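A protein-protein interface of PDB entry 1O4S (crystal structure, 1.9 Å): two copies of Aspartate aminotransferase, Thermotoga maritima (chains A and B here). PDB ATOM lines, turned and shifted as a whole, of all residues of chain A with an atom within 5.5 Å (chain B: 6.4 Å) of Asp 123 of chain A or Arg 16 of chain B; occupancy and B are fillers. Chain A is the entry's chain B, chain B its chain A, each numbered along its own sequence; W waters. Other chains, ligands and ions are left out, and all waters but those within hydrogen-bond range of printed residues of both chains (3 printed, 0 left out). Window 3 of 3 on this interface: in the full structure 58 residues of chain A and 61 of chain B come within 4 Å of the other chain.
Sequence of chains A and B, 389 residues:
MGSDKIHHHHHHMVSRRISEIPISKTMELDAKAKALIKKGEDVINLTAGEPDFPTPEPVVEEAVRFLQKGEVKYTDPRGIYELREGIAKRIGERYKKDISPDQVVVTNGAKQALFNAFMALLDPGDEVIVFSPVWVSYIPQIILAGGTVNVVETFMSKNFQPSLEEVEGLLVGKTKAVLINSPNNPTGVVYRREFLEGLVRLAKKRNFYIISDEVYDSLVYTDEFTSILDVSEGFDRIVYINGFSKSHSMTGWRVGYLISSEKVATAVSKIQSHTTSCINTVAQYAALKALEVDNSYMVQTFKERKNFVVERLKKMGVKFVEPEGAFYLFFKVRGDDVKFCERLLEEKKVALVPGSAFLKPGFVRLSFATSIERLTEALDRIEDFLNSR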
ATOM      1  N   LEU A 121      -7.151   2.421  10.439  1.00  0.00           N
ATOM      2  CA  LEU A 121      -6.200   3.506  10.506  1.00  0.00           C
ATOM      3  C   LEU A 121      -4.772   3.075  10.784  1.00  0.00           C
ATOM      4  O   LEU A 121      -3.855   3.852  10.537  1.00  0.00           O
ATOM      5  CB  LEU A 121      -6.599   4.495  11.610  1.00  0.00           C
ATOM      6  CG  LEU A 121      -7.940   5.184  11.476  1.00  0.00           C
ATOM      7  CD1 LEU A 121      -8.099   6.151  12.628  1.00  0.00           C
ATOM      8  CD2 LEU A 121      -8.056   5.869  10.126  1.00  0.00           C
ATOM      9  N   LEU A 122      -4.573   1.898  11.353  1.00  0.00           N
ATOM     10  CA  LEU A 122      -3.246   1.484  11.783  1.00  0.00           C
ATOM     11  C   LEU A 122      -2.583   0.553  10.773  1.00  0.00           C
ATOM     12  O   LEU A 122      -3.124  -0.491  10.425  1.00  0.00           O
ATOM     13  CB  LEU A 122      -3.295   0.769  13.122  1.00  0.00           C
ATOM     14  CG  LEU A 122      -3.834   1.493  14.347  1.00  0.00           C
ATOM     15  CD1 LEU A 122      -3.542   0.640  15.596  1.00  0.00           C
ATOM     16  CD2 LEU A 122      -3.246   2.923  14.494  1.00  0.00           C
ATOM     17  N   ASP A 123      -1.420   0.966  10.286  1.00  0.00           N
ATOM     18  CA  ASP A 123      -0.469   0.055   9.648  1.00  0.00           C
ATOM     19  C   ASP A 123       0.397  -0.589  10.734  1.00  0.00           C
ATOM     20  O   ASP A 123       0.557  -0.049  11.825  1.00  0.00           O
ATOM     21  CB  ASP A 123       0.431   0.808   8.663  1.00  0.00           C
ATOM     22  CG  ASP A 123      -0.317   1.313   7.467  1.00  0.00           C
ATOM     23  OD1 ASP A 123      -1.019   0.482   6.855  1.00  0.00           O
ATOM     24  OD2 ASP A 123      -0.260   2.508   7.075  1.00  0.00           O
ATOM     25  N   PRO A 124       0.970  -1.742  10.427  1.00  0.00           N
ATOM     26  CA  PRO A 124       1.849  -2.442  11.367  1.00  0.00           C
ATOM     27  C   PRO A 124       2.952  -1.572  11.948  1.00  0.00           C
ATOM     28  O   PRO A 124       3.653  -0.882  11.214  1.00  0.00           O
ATOM     29  CB  PRO A 124       2.442  -3.561  10.514  1.00  0.00           C
ATOM     30  CG  PRO A 124       1.364  -3.851   9.508  1.00  0.00           C
ATOM     31  CD  PRO A 124       0.816  -2.494   9.166  1.00  0.00           C
ATOM     32  N   GLY A 125       3.084  -1.617  13.265  1.00  0.00           N
ATOM     33  CA  GLY A 125       4.007  -0.768  13.995  1.00  0.00           C
ATOM     34  C   GLY A 125       3.536   0.655  14.343  1.00  0.00           C
ATOM     35  O   GLY A 125       4.200   1.318  15.151  1.00  0.00           O
ATOM     36  N   ASP A 126       2.451   1.142  13.729  1.00  0.00           N
ATOM     37  CA  ASP A 126       1.912   2.460  14.056  1.00  0.00           C
ATOM     38  C   ASP A 126       1.590   2.511  15.532  1.00  0.00           C
ATOM     39  O   ASP A 126       1.167   1.516  16.115  1.00  0.00           O
ATOM     40  CB  ASP A 126       0.648   2.785  13.264  1.00  0.00           C
ATOM     41  CG  ASP A 126       0.917   3.219  11.826  1.00  0.00           C
ATOM     42  OD1 ASP A 126       2.082   3.426  11.443  1.00  0.00           O
ATOM     43  OD2 ASP A 126      -0.002   3.429  11.013  1.00  0.00           O
ATOM     44  N   ALA A 145      -4.753  -5.299  15.850  1.00  0.00           N
ATOM     45  CA  ALA A 145      -4.628  -4.508  14.627  1.00  0.00           C
ATOM     46  C   ALA A 145      -3.190  -4.267  14.147  1.00  0.00           C
ATOM     47  O   ALA A 145      -3.006  -3.652  13.132  1.00  0.00           O
ATOM     48  CB  ALA A 145      -5.390  -3.179  14.766  1.00  0.00           C
ATOM     49  N   GLY A 146      -2.177  -4.744  14.855  1.00  0.00           N
ATOM     50  CA  GLY A 146      -0.805  -4.598  14.420  1.00  0.00           C
ATOM     51  C   GLY A 146      -0.098  -3.358  14.944  1.00  0.00           C
ATOM     52  O   GLY A 146       1.042  -3.107  14.590  1.00  0.00           O
ATOM     53  N   GLY A 147      -0.775  -2.565  15.761  1.00  0.00           N
ATOM     54  CA  GLY A 147      -0.205  -1.331  16.274  1.00  0.00           C
ATOM     55  C   GLY A 147       0.573  -1.556  17.543  1.00  0.00           C
ATOM     56  O   GLY A 147       0.592  -2.667  18.090  1.00  0.00           O
ATOM     57  N   LYS A 176       0.093   7.495  15.136  1.00  0.00           N
ATOM     58  CA  LYS A 176      -1.026   7.634  14.224  1.00  0.00           C
ATOM     59  C   LYS A 176      -2.308   8.136  14.915  1.00  0.00           C
ATOM     60  O   LYS A 176      -3.164   8.704  14.265  1.00  0.00           O
ATOM     61  CB  LYS A 176      -1.282   6.267  13.533  1.00  0.00           C
ATOM     62  CG  LYS A 176      -2.259   6.318  12.342  1.00  0.00           C
ATOM     63  CD  LYS A 176      -1.570   6.828  11.050  1.00  0.00           C
ATOM     64  CE  LYS A 176      -2.620   7.237   9.961  1.00  0.00           C
ATOM     65  NZ  LYS A 176      -3.247   6.092   9.165  1.00  0.00           N
ATOM     66  N   VAL B  14      -5.209   6.212   6.501  1.00  0.00           N
ATOM     67  CA  VAL B  14      -5.956   4.922   6.212  1.00  0.00           C
ATOM     68  C   VAL B  14      -4.994   3.750   5.919  1.00  0.00           C
ATOM     69  O   VAL B  14      -4.166   3.824   5.035  1.00  0.00           O
ATOM     70  CB  VAL B  14      -7.052   5.087   5.074  1.00  0.00           C
ATOM     71  CG1 VAL B  14      -7.500   3.735   4.487  1.00  0.00           C
ATOM     72  CG2 VAL B  14      -8.286   5.833   5.606  1.00  0.00           C
ATOM     73  N   SER B  15      -5.138   2.658   6.650  1.00  0.00           N
ATOM     74  CA  SER B  15      -4.213   1.546   6.554  1.00  0.00           C
ATOM     75  C   SER B  15      -4.096   0.923   5.154  1.00  0.00           C
ATOM     76  O   SER B  15      -5.071   0.830   4.380  1.00  0.00           O
ATOM     77  CB  SER B  15      -4.535   0.479   7.597  1.00  0.00           C
ATOM     78  OG  SER B  15      -5.737  -0.147   7.291  1.00  0.00           O
ATOM     79  N   ARG B  16      -2.861   0.510   4.853  1.00  0.00           N
ATOM     80  CA  ARG B  16      -2.498  -0.120   3.584  1.00  0.00           C
ATOM     81  C   ARG B  16      -3.338  -1.333   3.282  1.00  0.00           C
ATOM     82  O   ARG B  16      -3.746  -1.488   2.158  1.00  0.00           O
ATOM     83  CB  ARG B  16      -1.011  -0.522   3.565  1.00  0.00           C
ATOM     84  CG  ARG B  16      -0.068   0.608   3.195  1.00  0.00           C
ATOM     85  CD  ARG B  16       1.407   0.173   3.116  1.00  0.00           C
ATOM     86  NE  ARG B  16       2.198   0.640   4.264  1.00  0.00           N
ATOM     87  CZ  ARG B  16       2.594  -0.105   5.313  1.00  0.00           C
ATOM     88  NH1 ARG B  16       2.298  -1.408   5.412  1.00  0.00           N
ATOM     89  NH2 ARG B  16       3.309   0.482   6.275  1.00  0.00           N
ATOM     90  N   ARG B  17      -3.572  -2.187   4.270  1.00  0.00           N
ATOM     91  CA  ARG B  17      -4.406  -3.391   4.095  1.00  0.00           C
ATOM     92  C   ARG B  17      -5.806  -3.160   3.494  1.00  0.00           C
ATOM     93  O   ARG B  17      -6.303  -4.004   2.770  1.00  0.00           O
ATOM     94  CB  ARG B  17      -4.570  -4.113   5.425  1.00  0.00           C
ATOM     95  CG  ARG B  17      -4.928  -3.155   6.528  1.00  0.00           C
ATOM     96  CD  ARG B  17      -5.772  -3.691   7.602  1.00  0.00           C
ATOM     97  NE  ARG B  17      -5.030  -4.501   8.545  1.00  0.00           N
ATOM     98  CZ  ARG B  17      -4.489  -4.066   9.679  1.00  0.00           C
ATOM     99  NH1 ARG B  17      -4.547  -2.797  10.069  1.00  0.00           N
ATOM    100  NH2 ARG B  17      -3.870  -4.952  10.449  1.00  0.00           N
ATOM    101  N   ILE B  18      -6.428  -2.019   3.779  1.00  0.00           N
ATOM    102  CA  ILE B  18      -7.729  -1.686   3.198  1.00  0.00           C
ATOM    103  C   ILE B  18      -7.615  -1.548   1.663  1.00  0.00           C
ATOM    104  O   ILE B  18      -8.498  -2.031   0.946  1.00  0.00           O
ATOM    105  CB  ILE B  18      -8.345  -0.400   3.864  1.00  0.00           C
ATOM    106  CG1 ILE B  18      -9.180  -0.739   5.099  1.00  0.00           C
ATOM    107  CG2 ILE B  18      -9.320   0.303   2.918  1.00  0.00           C
ATOM    108  CD1 ILE B  18      -8.504  -1.586   6.093  1.00  0.00           C
ATOM    109  N   SER B  19      -6.554  -0.882   1.178  1.00  0.00           N
ATOM    110  CA  SER B  19      -6.225  -0.828  -0.271  1.00  0.00           C
ATOM    111  C   SER B  19      -5.825  -2.162  -0.880  1.00  0.00           C
ATOM    112  O   SER B  19      -5.905  -2.335  -2.093  1.00  0.00           O
ATOM    113  CB  SER B  19      -5.069   0.119  -0.546  1.00  0.00           C
ATOM    114  OG  SER B  19      -5.481   1.444  -0.276  1.00  0.00           O
ATOM    115  N   GLU B  20      -5.351  -3.091  -0.051  1.00  0.00           N
ATOM    116  CA  GLU B  20      -5.000  -4.409  -0.550  1.00  0.00           C
ATOM    117  C   GLU B  20      -6.253  -5.225  -0.804  1.00  0.00           C
ATOM    118  O   GLU B  20      -6.197  -6.174  -1.565  1.00  0.00           O
ATOM    119  CB  GLU B  20      -4.028  -5.126   0.388  1.00  0.00           C
ATOM    120  CG  GLU B  20      -2.587  -4.611   0.256  1.00  0.00           C
ATOM    121  CD  GLU B  20      -1.721  -4.852   1.496  1.00  0.00           C
ATOM    122  OE1 GLU B  20      -0.659  -4.174   1.615  1.00  0.00           O
ATOM    123  OE2 GLU B  20      -2.087  -5.684   2.373  1.00  0.00           O
ATOM    124  N   ILE B  21      -7.379  -4.848  -0.191  1.00  0.00           N
ATOM    125  CA  ILE B  21      -8.638  -5.588  -0.388  1.00  0.00           C
ATOM    126  C   ILE B  21      -9.047  -5.468  -1.858  1.00  0.00           C
ATOM    127  O   ILE B  21      -9.040  -4.373  -2.420  1.00  0.00           O
ATOM    128  CB  ILE B  21      -9.765  -5.102   0.552  1.00  0.00           C
ATOM    129  CG1 ILE B  21      -9.432  -5.462   2.011  1.00  0.00           C
ATOM    130  CG2 ILE B  21     -11.084  -5.781   0.201  1.00  0.00           C
ATOM    131  CD1 ILE B  21     -10.344  -4.795   3.007  1.00  0.00           C
HETATM  132  O   HOH W   1      -1.607  -3.398  10.576  1.00  0.00           O
HETATM  133  O   HOH W   2       4.228  -0.728   8.668  1.00  0.00           O
HETATM  134  O   HOH W   3      -1.644  -1.983   6.953  1.00  0.00           O
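The backbone NH of Asp 123 of chain A sits at hydrogen-bond distance from the side-chain carboxylate of Asp 126 of chain A (2.9 Å). O of Leu 121 of chain A sits at hydrogen-bond distance from NZ of Lys 176 of chain A, 2.7 Å away.
Of the 8 printed residues of chain B, 4 touch a printed residue of chain A. Printed residues of chain B that touch a printed residue of chain A: Val 14, Ser 15, Arg 16 and Arg 17. Among the printed residues, 6 pairs touch across the chains. Among the printed residues, no Asp or Glu carboxylate lies within 4 Å of a Lys or Arg side-chain nitrogen of the other chain.
The side-chain carboxylate (OD1) of Asp 123 of chain A is in hydrogen-bond range of the backbone NH (N) of Arg 16 of chain B. The guanidinium group (NH2) of Arg 17 of chain B sits at hydrogen-bond distance from the backbone carbonyl oxygen (O) of Ala 145 of chain A (3.1 Å). NZ of Lys 176 of chain A lies close to N of Val 14 of chain B (3.3 Å). O of Leu 122 of chain A is in hydrogen-bond range of NH1 of Arg 17 of chain B.
No position is printed for both chains. Of the 6 pairs that touch across the chains among the printed residues, none has its exchanged pair printed and touching as well.
O of Leu 122 of chain A touches CB of Ser 15 of chain B (3.3 Å). Asp 123 of chain A touches Ser 15 of chain B (OD1 to CA, 3.4 Å).
Asp 123 of chain A touches just these residues of chain B: Ser 15 and Arg 16. Arg 16 of chain B touches just one residue of chain A: Asp 123. Printed residues of chain B within 4 Å of Leu 122 of chain A: Ser 15 and Arg 17. Of the printed residues of chain A, Ser 15 of chain B touches Leu 122 and Asp 123. Printed residues of chain B within 4 Å of Lys 176 of chain A: Val 14 (3.3 Å). Of the printed residues of chain B, Ala 145 of chain A touches Arg 17 (3.1 Å). Gly 147 of chain A touches none of the printed residues of chain B. Ser 19 of chain B touches none of the printed residues of chain A.
Water W3 lies within hydrogen-bond range of the side-chain carboxylate of Asp 123 of chain A (2.5 Å), the backbone NH of Arg 17 of chain B (3.3 Å) and the backbone NH of Arg 16 of chain B (3.5 Å). Water W2 lies within hydrogen-bond range of the backbone carbonyl oxygen (O) of Pro 124 of chain A (2.6 Å) and the guanidinium group (NH2) of Arg 16 of chain B (2.8 Å). Water W1 lies within hydrogen-bond range of NH2 of Arg 17 of chain B (2.7 Å), O of Ala 145 of chain A (2.9 Å) and O of Leu 122 of chain A (3.3 Å).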
